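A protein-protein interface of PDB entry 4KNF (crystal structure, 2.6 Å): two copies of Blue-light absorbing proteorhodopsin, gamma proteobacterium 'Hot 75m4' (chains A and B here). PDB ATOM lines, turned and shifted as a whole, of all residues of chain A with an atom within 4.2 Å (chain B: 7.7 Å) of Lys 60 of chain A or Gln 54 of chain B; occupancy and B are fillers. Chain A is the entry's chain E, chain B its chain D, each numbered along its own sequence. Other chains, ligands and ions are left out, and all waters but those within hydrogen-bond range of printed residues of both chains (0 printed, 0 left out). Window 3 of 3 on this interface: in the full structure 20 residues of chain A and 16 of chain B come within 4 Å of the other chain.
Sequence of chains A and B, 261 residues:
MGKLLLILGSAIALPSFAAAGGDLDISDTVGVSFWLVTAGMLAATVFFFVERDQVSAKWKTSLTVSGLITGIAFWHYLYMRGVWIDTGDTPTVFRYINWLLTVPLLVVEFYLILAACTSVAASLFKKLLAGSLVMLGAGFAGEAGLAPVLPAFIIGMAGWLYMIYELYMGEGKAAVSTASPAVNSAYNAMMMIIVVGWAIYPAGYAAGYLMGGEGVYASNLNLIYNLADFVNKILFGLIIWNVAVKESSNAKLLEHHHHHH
The backbone carbonyl oxygen of Val 55 of chain A is in hydrogen-bond range of the side-chain amino group of Lys 60 of chain A, at 2.7 Å. OE2 of Glu 51 of chain B sits at hydrogen-bond distance from NE1 of Trp 241 of chain B (3.2 Å). The backbone carbonyl oxygen (O) of Arg 52 of chain A sits at hydrogen-bond distance from the side-chain amino group (NZ) of Lys 60 of chain A (3.1 Å). NH1 of Arg 52 of chain A lies within hydrogen-bond range of OG1 of Thr 64 of chain A (2.8 Å). The side-chain hydroxyl of Thr 64 of chain A is in hydrogen-bond range of the backbone carbonyl oxygen of Lys 60 of chain A (2.9 Å).
Among the printed residues, pairs that only touch across the chains: Lys 60 of chain A with Asp 53 of chain B, Lys 60 of chain A with Gln 54 of chain B, Thr 61 of chain A with Phe 47 of chain B, Thr 61 of chain A with Trp 241 of chain B and Thr 64 of chain A with Val 50 of chain B.
Hydrophobic or aromatic side chains of chain B that line the printed part of chain A: Phe 47, Val 50 and Trp 241. Of the 11 printed residues of chain A, 5 touch a printed residue of chain B. Among the printed residues, Asp or Glu carboxylates within 4 Å of a Lys or Arg side-chain nitrogen of the other chain: Arg 52 of chain A with Glu 51 of chain B (3.2 Å) and Arg 52 of chain A with Asp 53 of chain B (2.6 Å).
Printed residues of chain B within 4 Å of Arg 52 of chain A: Val 50 (3.3 Å), Glu 51 (3.2 Å) and Asp 53 (2.6 Å). Of the printed residues of chain B, Ala 57 of chain A touches Gln 54. Of chain B, only Asp 53 and Gln 54 come within 4 Å of Lys 60 of chain A. Of the printed residues of chain A, Phe 47 of chain B touches Thr 61. Gln 54 of chain B touches just these residues of chain A: Ala 57 (3.1 Å), Lys 60 (3.2 Å) and Thr 61 (3.2 Å). The nearest residue of chain B that does not touch Lys 60 of chain A is Glu 51 of chain B (4.3 Å). The nearest printed residue of chain A that does not touch Asp 53 of chain B is Ala 57 of chain A (6.2 Å).
Positions printed for both chains: 52, 55, 56, 59, 60 and 63. Of the 12 pairs that touch across the chains among the printed residues, none has its exchanged pair printed and touching as well.
OE2 of Glu 51 of chain B is in hydrogen-bond range of OG1 of Thr 61 of chain A (2.8 Å). OD2 of Asp 53 of chain B lies within salt-bridge range of NH2 of Arg 52 of chain A (2.6 Å). O of Ala 57 of chain A is in hydrogen-bond range of NE2 of Gln 54 of chain B, 3.1 Å away. The side-chain carboxylate (OE1) of Glu 51 of chain B is in salt-bridge range of the guanidinium group (NH1) of Arg 52 of chain A (3.2 Å). The backbone carbonyl oxygen (O) of Val 50 of chain B sits at hydrogen-bond distance from the guanidinium group (NH2) of Arg 52 of chain A. OG1 of Thr 64 of chain A is in hydrogen-bond range of OE1 of Glu 51 of chain B, 2.7 Å away. The side-chain amide nitrogen (NE2) of Gln 54 of chain B sits at hydrogen-bond distance from the side-chain hydroxyl (OG1) of Thr 61 of chain A (3.2 Å).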
ATOM      1  N   ARG A  52      29.880  -4.987  -5.161  1.00  0.00           N
ATOM      2  CA  ARG A  52      28.664  -5.526  -5.745  1.00  0.00           C
ATOM      3  C   ARG A  52      27.640  -5.870  -4.670  1.00  0.00           C
ATOM      4  O   ARG A  52      26.432  -5.839  -4.915  1.00  0.00           O
ATOM      5  CB  ARG A  52      28.993  -6.740  -6.586  1.00  0.00           C
ATOM      6  CG  ARG A  52      29.131  -6.403  -8.064  1.00  0.00           C
ATOM      7  CD  ARG A  52      29.745  -7.554  -8.841  1.00  0.00           C
ATOM      8  NE  ARG A  52      29.200  -8.804  -8.334  1.00  0.00           N
ATOM      9  CZ  ARG A  52      28.115  -9.381  -8.813  1.00  0.00           C
ATOM     10  NH1 ARG A  52      27.478  -8.841  -9.830  1.00  0.00           N
ATOM     11  NH2 ARG A  52      27.685 -10.501  -8.289  1.00  0.00           N
ATOM     12  N   VAL A  55      25.062  -3.066  -3.913  1.00  0.00           N
ATOM     13  CA  VAL A  55      23.992  -2.811  -4.859  1.00  0.00           C
ATOM     14  C   VAL A  55      23.124  -4.063  -5.027  1.00  0.00           C
ATOM     15  O   VAL A  55      23.575  -5.197  -4.790  1.00  0.00           O
ATOM     16  CB  VAL A  55      24.507  -2.326  -6.236  1.00  0.00           C
ATOM     17  CG1 VAL A  55      25.462  -1.145  -6.080  1.00  0.00           C
ATOM     18  CG2 VAL A  55      25.164  -3.462  -7.013  1.00  0.00           C
ATOM     19  N   SER A  56      21.875  -3.829  -5.431  1.00  0.00           N
ATOM     20  CA  SER A  56      20.880  -4.865  -5.613  1.00  0.00           C
ATOM     21  C   SER A  56      21.051  -5.551  -6.974  1.00  0.00           C
ATOM     22  O   SER A  56      21.849  -5.110  -7.805  1.00  0.00           O
ATOM     23  CB  SER A  56      19.508  -4.227  -5.545  1.00  0.00           C
ATOM     24  OG  SER A  56      19.255  -3.570  -6.762  1.00  0.00           O
ATOM     25  N   ALA A  57      20.274  -6.607  -7.206  1.00  0.00           N
ATOM     26  CA  ALA A  57      20.399  -7.410  -8.420  1.00  0.00           C
ATOM     27  C   ALA A  57      20.317  -6.560  -9.682  1.00  0.00           C
ATOM     28  O   ALA A  57      21.091  -6.772 -10.623  1.00  0.00           O
ATOM     29  CB  ALA A  57      19.378  -8.539  -8.442  1.00  0.00           C
ATOM     30  N   LYS A  58      19.401  -5.590  -9.695  1.00  0.00           N
ATOM     31  CA  LYS A  58      19.329  -4.623 -10.804  1.00  0.00           C
ATOM     32  C   LYS A  58      20.701  -4.134 -11.279  1.00  0.00           C
ATOM     33  O   LYS A  58      20.912  -3.994 -12.472  1.00  0.00           O
ATOM     34  CB  LYS A  58      18.473  -3.408 -10.435  1.00  0.00           C
ATOM     35  CG  LYS A  58      16.999  -3.551 -10.785  1.00  0.00           C
ATOM     36  CD  LYS A  58      16.238  -2.274 -10.475  1.00  0.00           C
ATOM     37  CE  LYS A  58      15.988  -2.147  -8.987  1.00  0.00           C
ATOM     38  NZ  LYS A  58      16.303  -0.765  -8.548  1.00  0.00           N
ATOM     39  N   TRP A  59      21.630  -3.900 -10.351  1.00  0.00           N
ATOM     40  CA  TRP A  59      22.877  -3.189 -10.654  1.00  0.00           C
ATOM     41  C   TRP A  59      24.133  -4.057 -10.672  1.00  0.00           C
ATOM     42  O   TRP A  59      25.193  -3.624 -11.139  1.00  0.00           O
ATOM     43  CB  TRP A  59      23.090  -2.051  -9.657  1.00  0.00           C
ATOM     44  CG  TRP A  59      22.031  -1.065  -9.703  1.00  0.00           C
ATOM     45  CD1 TRP A  59      20.939  -0.984  -8.879  1.00  0.00           C
ATOM     46  CD2 TRP A  59      21.918  -0.003 -10.639  1.00  0.00           C
ATOM     47  NE1 TRP A  59      20.161   0.085  -9.241  1.00  0.00           N
ATOM     48  CE2 TRP A  59      20.734   0.703 -10.324  1.00  0.00           C
ATOM     49  CE3 TRP A  59      22.702   0.430 -11.716  1.00  0.00           C
ATOM     50  CZ2 TRP A  59      20.315   1.823 -11.052  1.00  0.00           C
ATOM     51  CZ3 TRP A  59      22.281   1.540 -12.441  1.00  0.00           C
ATOM     52  CH2 TRP A  59      21.094   2.222 -12.103  1.00  0.00           C
ATOM     53  N   LYS A  60      24.021  -5.261 -10.138  1.00  0.00           N
ATOM     54  CA  LYS A  60      25.180  -6.105  -9.948  1.00  0.00           C
ATOM     55  C   LYS A  60      25.953  -6.347 -11.258  1.00  0.00           C
ATOM     56  O   LYS A  60      27.158  -6.116 -11.304  1.00  0.00           O
ATOM     57  CB  LYS A  60      24.798  -7.413  -9.249  1.00  0.00           C
ATOM     58  CG  LYS A  60      24.713  -7.325  -7.741  1.00  0.00           C
ATOM     59  CD  LYS A  60      24.059  -8.609  -7.218  1.00  0.00           C
ATOM     60  CE  LYS A  60      24.400  -8.953  -5.771  1.00  0.00           C
ATOM     61  NZ  LYS A  60      24.086  -7.824  -4.859  1.00  0.00           N
ATOM     62  N   THR A  61      25.260  -6.765 -12.320  1.00  0.00           N
ATOM     63  CA  THR A  61      25.920  -7.003 -13.629  1.00  0.00           C
ATOM     64  C   THR A  61      26.697  -5.776 -14.166  1.00  0.00           C
ATOM     65  O   THR A  61      27.845  -5.895 -14.634  1.00  0.00           O
ATOM     66  CB  THR A  61      24.929  -7.560 -14.670  1.00  0.00           C
ATOM     67  OG1 THR A  61      24.209  -8.642 -14.079  1.00  0.00           O
ATOM     68  CG2 THR A  61      25.652  -8.104 -15.873  1.00  0.00           C
ATOM     69  N   SER A  62      26.073  -4.605 -14.067  1.00  0.00           N
ATOM     70  CA  SER A  62      26.746  -3.336 -14.329  1.00  0.00           C
ATOM     71  C   SER A  62      28.116  -3.210 -13.692  1.00  0.00           C
ATOM     72  O   SER A  62      29.056  -2.779 -14.360  1.00  0.00           O
ATOM     73  CB  SER A  62      25.894  -2.171 -13.864  1.00  0.00           C
ATOM     74  OG  SER A  62      25.215  -1.677 -14.984  1.00  0.00           O
ATOM     75  N   LEU A  63      28.206  -3.551 -12.398  1.00  0.00           N
ATOM     76  CA  LEU A  63      29.443  -3.433 -11.652  1.00  0.00           C
ATOM     77  C   LEU A  63      30.453  -4.499 -12.088  1.00  0.00           C
ATOM     78  O   LEU A  63      31.666  -4.233 -12.128  1.00  0.00           O
ATOM     79  CB  LEU A  63      29.191  -3.491 -10.159  1.00  0.00           C
ATOM     80  CG  LEU A  63      28.538  -2.284  -9.469  1.00  0.00           C
ATOM     81  CD1 LEU A  63      28.915  -2.275  -7.997  1.00  0.00           C
ATOM     82  CD2 LEU A  63      28.900  -0.958 -10.105  1.00  0.00           C
ATOM     83  N   THR A  64      29.927  -5.669 -12.465  1.00  0.00           N
ATOM     84  CA  THR A  64      30.707  -6.747 -13.028  1.00  0.00           C
ATOM     85  C   THR A  64      31.349  -6.340 -14.349  1.00  0.00           C
ATOM     86  O   THR A  64      32.568  -6.547 -14.552  1.00  0.00           O
ATOM     87  CB  THR A  64      29.858  -8.017 -13.213  1.00  0.00           C
ATOM     88  OG1 THR A  64      29.051  -8.225 -12.047  1.00  0.00           O
ATOM     89  CG2 THR A  64      30.751  -9.241 -13.412  1.00  0.00           C
ATOM     90  N   PHE B  47      33.368 -13.332 -15.306  1.00  0.00           N
ATOM     91  CA  PHE B  47      31.961 -13.050 -15.491  1.00  0.00           C
ATOM     92  C   PHE B  47      31.082 -14.184 -14.939  1.00  0.00           C
ATOM     93  O   PHE B  47      30.236 -13.922 -14.095  1.00  0.00           O
ATOM     94  CB  PHE B  47      31.618 -12.706 -16.971  1.00  0.00           C
ATOM     95  CG  PHE B  47      30.159 -12.313 -17.170  1.00  0.00           C
ATOM     96  CD1 PHE B  47      29.742 -11.007 -16.978  1.00  0.00           C
ATOM     97  CD2 PHE B  47      29.206 -13.267 -17.510  1.00  0.00           C
ATOM     98  CE1 PHE B  47      28.394 -10.648 -17.116  1.00  0.00           C
ATOM     99  CE2 PHE B  47      27.846 -12.923 -17.648  1.00  0.00           C
ATOM    100  CZ  PHE B  47      27.442 -11.605 -17.455  1.00  0.00           C
ATOM    101  N   PHE B  49      31.733 -16.908 -12.976  1.00  0.00           N
ATOM    102  CA  PHE B  49      31.860 -17.140 -11.534  1.00  0.00           C
ATOM    103  C   PHE B  49      31.232 -16.063 -10.663  1.00  0.00           C
ATOM    104  O   PHE B  49      30.578 -16.374  -9.670  1.00  0.00           O
ATOM    105  CB  PHE B  49      33.299 -17.404 -11.118  1.00  0.00           C
ATOM    106  CG  PHE B  49      33.745 -18.793 -11.434  1.00  0.00           C
ATOM    107  CD1 PHE B  49      33.004 -19.888 -10.980  1.00  0.00           C
ATOM    108  CD2 PHE B  49      34.888 -19.020 -12.186  1.00  0.00           C
ATOM    109  CE1 PHE B  49      33.405 -21.182 -11.267  1.00  0.00           C
ATOM    110  CE2 PHE B  49      35.289 -20.315 -12.475  1.00  0.00           C
ATOM    111  CZ  PHE B  49      34.551 -21.393 -12.016  1.00  0.00           C
ATOM    112  N   VAL B  50      31.432 -14.806 -11.034  1.00  0.00           N
ATOM    113  CA  VAL B  50      30.946 -13.702 -10.233  1.00  0.00           C
ATOM    114  C   VAL B  50      29.415 -13.643 -10.265  1.00  0.00           C
ATOM    115  O   VAL B  50      28.780 -13.477  -9.232  1.00  0.00           O
ATOM    116  CB  VAL B  50      31.577 -12.365 -10.662  1.00  0.00           C
ATOM    117  CG1 VAL B  50      30.898 -11.200  -9.956  1.00  0.00           C
ATOM    118  CG2 VAL B  50      33.077 -12.374 -10.368  1.00  0.00           C
ATOM    119  N   GLU B  51      28.842 -13.846 -11.447  1.00  0.00           N
ATOM    120  CA  GLU B  51      27.413 -13.648 -11.678  1.00  0.00           C
ATOM    121  C   GLU B  51      26.533 -14.728 -11.049  1.00  0.00           C
ATOM    122  O   GLU B  51      25.313 -14.592 -11.028  1.00  0.00           O
ATOM    123  CB  GLU B  51      27.124 -13.566 -13.178  1.00  0.00           C
ATOM    124  CG  GLU B  51      27.535 -12.277 -13.841  1.00  0.00           C
ATOM    125  CD  GLU B  51      26.766 -11.090 -13.318  1.00  0.00           C
ATOM    126  OE1 GLU B  51      27.403 -10.207 -12.711  1.00  0.00           O
ATOM    127  OE2 GLU B  51      25.527 -11.039 -13.499  1.00  0.00           O
ATOM    128  N   ARG B  52      27.151 -15.789 -10.535  1.00  0.00           N
ATOM    129  CA  ARG B  52      26.425 -16.870  -9.855  1.00  0.00           C
ATOM    130  C   ARG B  52      25.436 -16.409  -8.796  1.00  0.00           C
ATOM    131  O   ARG B  52      24.442 -17.106  -8.504  1.00  0.00           O
ATOM    132  CB  ARG B  52      27.392 -17.822  -9.200  1.00  0.00           C
ATOM    133  CG  ARG B  52      27.744 -18.958 -10.117  1.00  0.00           C
ATOM    134  CD  ARG B  52      28.920 -19.714  -9.566  1.00  0.00           C
ATOM    135  NE  ARG B  52      28.702 -19.923  -8.131  1.00  0.00           N
ATOM    136  CZ  ARG B  52      28.121 -20.990  -7.624  1.00  0.00           C
ATOM    137  NH1 ARG B  52      27.981 -21.090  -6.327  1.00  0.00           N
ATOM    138  NH2 ARG B  52      27.707 -21.959  -8.427  1.00  0.00           N
ATOM    139  N   ASP B  53      25.722 -15.248  -8.213  1.00  0.00           N
ATOM    140  CA  ASP B  53      24.909 -14.746  -7.147  1.00  0.00           C
ATOM    141  C   ASP B  53      23.685 -13.969  -7.671  1.00  0.00           C
ATOM    142  O   ASP B  53      22.910 -13.444  -6.887  1.00  0.00           O
ATOM    143  CB  ASP B  53      25.766 -13.898  -6.236  1.00  0.00           C
ATOM    144  CG  ASP B  53      26.252 -12.678  -6.921  1.00  0.00           C
ATOM    145  OD1 ASP B  53      26.096 -12.640  -8.172  1.00  0.00           O
ATOM    146  OD2 ASP B  53      26.775 -11.762  -6.227  1.00  0.00           O
ATOM    147  N   GLN B  54      23.549 -13.900  -8.994  1.00  0.00           N
ATOM    148  CA  GLN B  54      22.399 -13.319  -9.691  1.00  0.00           C
ATOM    149  C   GLN B  54      21.448 -14.385 -10.210  1.00  0.00           C
ATOM    150  O   GLN B  54      20.517 -14.063 -10.931  1.00  0.00           O
ATOM    151  CB  GLN B  54      22.861 -12.571 -10.923  1.00  0.00           C
ATOM    152  CG  GLN B  54      23.602 -11.291 -10.675  1.00  0.00           C
ATOM    153  CD  GLN B  54      22.665 -10.145 -10.489  1.00  0.00           C
ATOM    154  OE1 GLN B  54      22.159  -9.915  -9.394  1.00  0.00           O
ATOM    155  NE2 GLN B  54      22.428  -9.409 -11.557  1.00  0.00           N
ATOM    156  N   VAL B  55      21.720 -15.652  -9.904  1.00  0.00           N
ATOM    157  CA  VAL B  55      20.868 -16.770 -10.331  1.00  0.00           C
ATOM    158  C   VAL B  55      20.575 -17.656  -9.119  1.00  0.00           C
ATOM    159  O   VAL B  55      21.337 -17.666  -8.152  1.00  0.00           O
ATOM    160  CB  VAL B  55      21.509 -17.631 -11.455  1.00  0.00           C
ATOM    161  CG1 VAL B  55      22.023 -16.773 -12.603  1.00  0.00           C
ATOM    162  CG2 VAL B  55      22.627 -18.499 -10.918  1.00  0.00           C
ATOM    163  N   SER B  56      19.468 -18.390  -9.179  1.00  0.00           N
ATOM    164  CA  SER B  56      19.030 -19.276  -8.105  1.00  0.00           C
ATOM    165  C   SER B  56      19.848 -20.576  -8.031  1.00  0.00           C
ATOM    166  O   SER B  56      20.579 -20.934  -8.981  1.00  0.00           O
ATOM    167  CB  SER B  56      17.571 -19.637  -8.334  1.00  0.00           C
ATOM    168  OG  SER B  56      17.471 -20.596  -9.384  1.00  0.00           O
ATOM    169  N   TRP B  59      20.248 -22.844 -10.949  1.00  0.00           N
ATOM    170  CA  TRP B  59      21.136 -22.444 -12.064  1.00  0.00           C
ATOM    171  C   TRP B  59      22.633 -22.344 -11.736  1.00  0.00           C
ATOM    172  O   TRP B  59      23.467 -22.332 -12.648  1.00  0.00           O
ATOM    173  CB  TRP B  59      20.697 -21.118 -12.654  1.00  0.00           C
ATOM    174  CG  TRP B  59      19.316 -21.141 -13.189  1.00  0.00           C
ATOM    175  CD1 TRP B  59      18.172 -20.651 -12.576  1.00  0.00           C
ATOM    176  CD2 TRP B  59      18.900 -21.679 -14.446  1.00  0.00           C
ATOM    177  NE1 TRP B  59      17.080 -20.860 -13.389  1.00  0.00           N
ATOM    178  CE2 TRP B  59      17.495 -21.488 -14.538  1.00  0.00           C
ATOM    179  CE3 TRP B  59      19.570 -22.304 -15.501  1.00  0.00           C
ATOM    180  CZ2 TRP B  59      16.756 -21.905 -15.647  1.00  0.00           C
ATOM    181  CZ3 TRP B  59      18.834 -22.726 -16.596  1.00  0.00           C
ATOM    182  CH2 TRP B  59      17.437 -22.517 -16.663  1.00  0.00           C
ATOM    183  N   LYS B  60      22.964 -22.262 -10.449  1.00  0.00           N
ATOM    184  CA  LYS B  60      24.305 -21.972 -10.026  1.00  0.00           C
ATOM    185  C   LYS B  60      25.378 -22.954 -10.558  1.00  0.00           C
ATOM    186  O   LYS B  60      26.461 -22.523 -10.995  1.00  0.00           O
ATOM    187  CB  LYS B  60      24.352 -21.869  -8.513  1.00  0.00           C
ATOM    188  CG  LYS B  60      23.826 -20.559  -7.954  1.00  0.00           C
ATOM    189  CD  LYS B  60      24.171 -20.457  -6.476  1.00  0.00           C
ATOM    190  CE  LYS B  60      24.199 -19.014  -5.988  1.00  0.00           C
ATOM    191  NZ  LYS B  60      22.839 -18.412  -5.928  1.00  0.00           N
ATOM    192  N   LEU B  63      26.393 -22.210 -14.110  1.00  0.00           N
ATOM    193  CA  LEU B  63      27.344 -21.133 -14.234  1.00  0.00           C
ATOM    194  C   LEU B  63      28.762 -21.575 -13.821  1.00  0.00           C
ATOM    195  O   LEU B  63      29.750 -21.147 -14.429  1.00  0.00           O
ATOM    196  CB  LEU B  63      26.867 -19.920 -13.464  1.00  0.00           C
ATOM    197  CG  LEU B  63      25.880 -18.997 -14.178  1.00  0.00           C
ATOM    198  CD1 LEU B  63      24.470 -19.576 -14.171  1.00  0.00           C
ATOM    199  CD2 LEU B  63      25.864 -17.630 -13.499  1.00  0.00           C
ATOM    200  N   TRP B 241      23.412 -17.951 -19.051  1.00  0.00           N
ATOM    201  CA  TRP B 241      23.326 -16.882 -18.068  1.00  0.00           C
ATOM    202  C   TRP B 241      22.049 -16.041 -18.227  1.00  0.00           C
ATOM    203  O   TRP B 241      21.434 -15.660 -17.229  1.00  0.00           O
ATOM    204  CB  TRP B 241      24.536 -15.990 -18.173  1.00  0.00           C
ATOM    205  CG  TRP B 241      24.468 -14.759 -17.292  1.00  0.00           C
ATOM    206  CD1 TRP B 241      24.735 -14.678 -15.938  1.00  0.00           C
ATOM    207  CD2 TRP B 241      24.139 -13.421 -17.714  1.00  0.00           C
ATOM    208  NE1 TRP B 241      24.587 -13.361 -15.500  1.00  0.00           N
ATOM    209  CE2 TRP B 241      24.224 -12.582 -16.570  1.00  0.00           C
ATOM    210  CE3 TRP B 241      23.786 -12.855 -18.949  1.00  0.00           C
ATOM    211  CZ2 TRP B 241      23.967 -11.222 -16.631  1.00  0.00           C
ATOM    212  CZ3 TRP B 241      23.528 -11.496 -19.006  1.00  0.00           C
ATOM    213  CH2 TRP B 241      23.616 -10.694 -17.853  1.00  0.00           C
ATOM    214  N   ALA B 244      18.991 -18.044 -17.055  1.00  0.00           N
ATOM    215  CA  ALA B 244      19.000 -18.188 -15.596  1.00  0.00           C
ATOM    216  C   ALA B 244      18.628 -16.897 -14.888  1.00  0.00           C
ATOM    217  O   ALA B 244      17.912 -16.915 -13.881  1.00  0.00           O
ATOM    218  CB  ALA B 244      20.359 -18.659 -15.123  1.00  0.00           C
ATOM    219  N   VAL B 245      19.116 -15.781 -15.422  1.00  0.00           N
ATOM    220  CA  VAL B 245      18.889 -14.477 -14.814  1.00  0.00           C
ATOM    221  C   VAL B 245      17.425 -14.085 -14.918  1.00  0.00           C
ATOM    222  O   VAL B 245      16.824 -13.624 -13.939  1.00  0.00           O
ATOM    223  CB  VAL B 245      19.792 -13.390 -15.429  1.00  0.00           C
ATOM    224  CG1 VAL B 245      19.207 -12.005 -15.196  1.00  0.00           C
ATOM    225  CG2 VAL B 245      21.186 -13.469 -14.824  1.00  0.00           C
ATOM    226  N   LYS B 246      16.857 -14.282 -16.102  1.00  0.00           N
ATOM    227  CA  LYS B 246      15.456 -13.991 -16.315  1.00  0.00           C
ATOM    228  C   LYS B 246      14.584 -14.828 -15.383  1.00  0.00           C
ATOM    229  O   LYS B 246      13.702 -14.276 -14.709  1.00  0.00           O
ATOM    230  CB  LYS B 246      15.078 -14.220 -17.768  1.00  0.00           C
ATOM    231  CG  LYS B 246      15.351 -13.025 -18.645  1.00  0.00           C
ATOM    232  CD  LYS B 246      14.871 -13.337 -20.047  1.00  0.00           C
ATOM    233  CE  LYS B 246      15.759 -12.697 -21.096  1.00  0.00           C
ATOM    234  NZ  LYS B 246      15.570 -13.406 -22.394  1.00  0.00           N
ATOM    235  N   GLU B 247      14.855 -16.136 -15.319  1.00  0.00           N
ATOM    236  CA  GLU B 247      14.034 -17.054 -14.526  1.00  0.00           C
ATOM    237  C   GLU B 247      14.104 -16.770 -13.032  1.00  0.00           C
ATOM    238  O   GLU B 247      13.110 -16.894 -12.324  1.00  0.00           O
ATOM    239  CB  GLU B 247      14.408 -18.505 -14.800  1.00  0.00           C
ATOM    240  CG  GLU B 247      13.392 -19.513 -14.292  1.00  0.00           C
ATOM    241  CD  GLU B 247      13.703 -20.083 -12.913  1.00  0.00           C
ATOM    242  OE1 GLU B 247      13.222 -21.199 -12.633  1.00  0.00           O
ATOM    243  OE2 GLU B 247      14.412 -19.452 -12.100  1.00  0.00           O
ATOM    244  N   SER B 248      15.278 -16.392 -12.556  1.00  0.00           N
ATOM    245  CA  SER B 248      15.487 -16.196 -11.130  1.00  0.00           C
ATOM    246  C   SER B 248      14.771 -14.945 -10.614  1.00  0.00           C
ATOM    247  O   SER B 248      14.244 -14.942  -9.497  1.00  0.00           O
ATOM    248  CB  SER B 248      16.989 -16.172 -10.803  1.00  0.00           C
ATOM    249  OG  SER B 248      17.605 -17.388 -11.226  1.00  0.00           O
ATOM    250  N   SER B 249      14.745 -13.894 -11.429  1.00  0.00           N
ATOM    251  CA  SER B 249      14.080 -12.652 -11.046  1.00  0.00           C
ATOM    252  C   SER B 249      12.548 -12.760 -11.225  1.00  0.00           C
ATOM    253  O   SER B 249      11.778 -12.060 -10.554  1.00  0.00           O
ATOM    254  CB  SER B 249      14.641 -11.490 -11.848  1.00  0.00           C
ATOM    255  OG  SER B 249      14.507 -11.763 -13.226  1.00  0.00           O
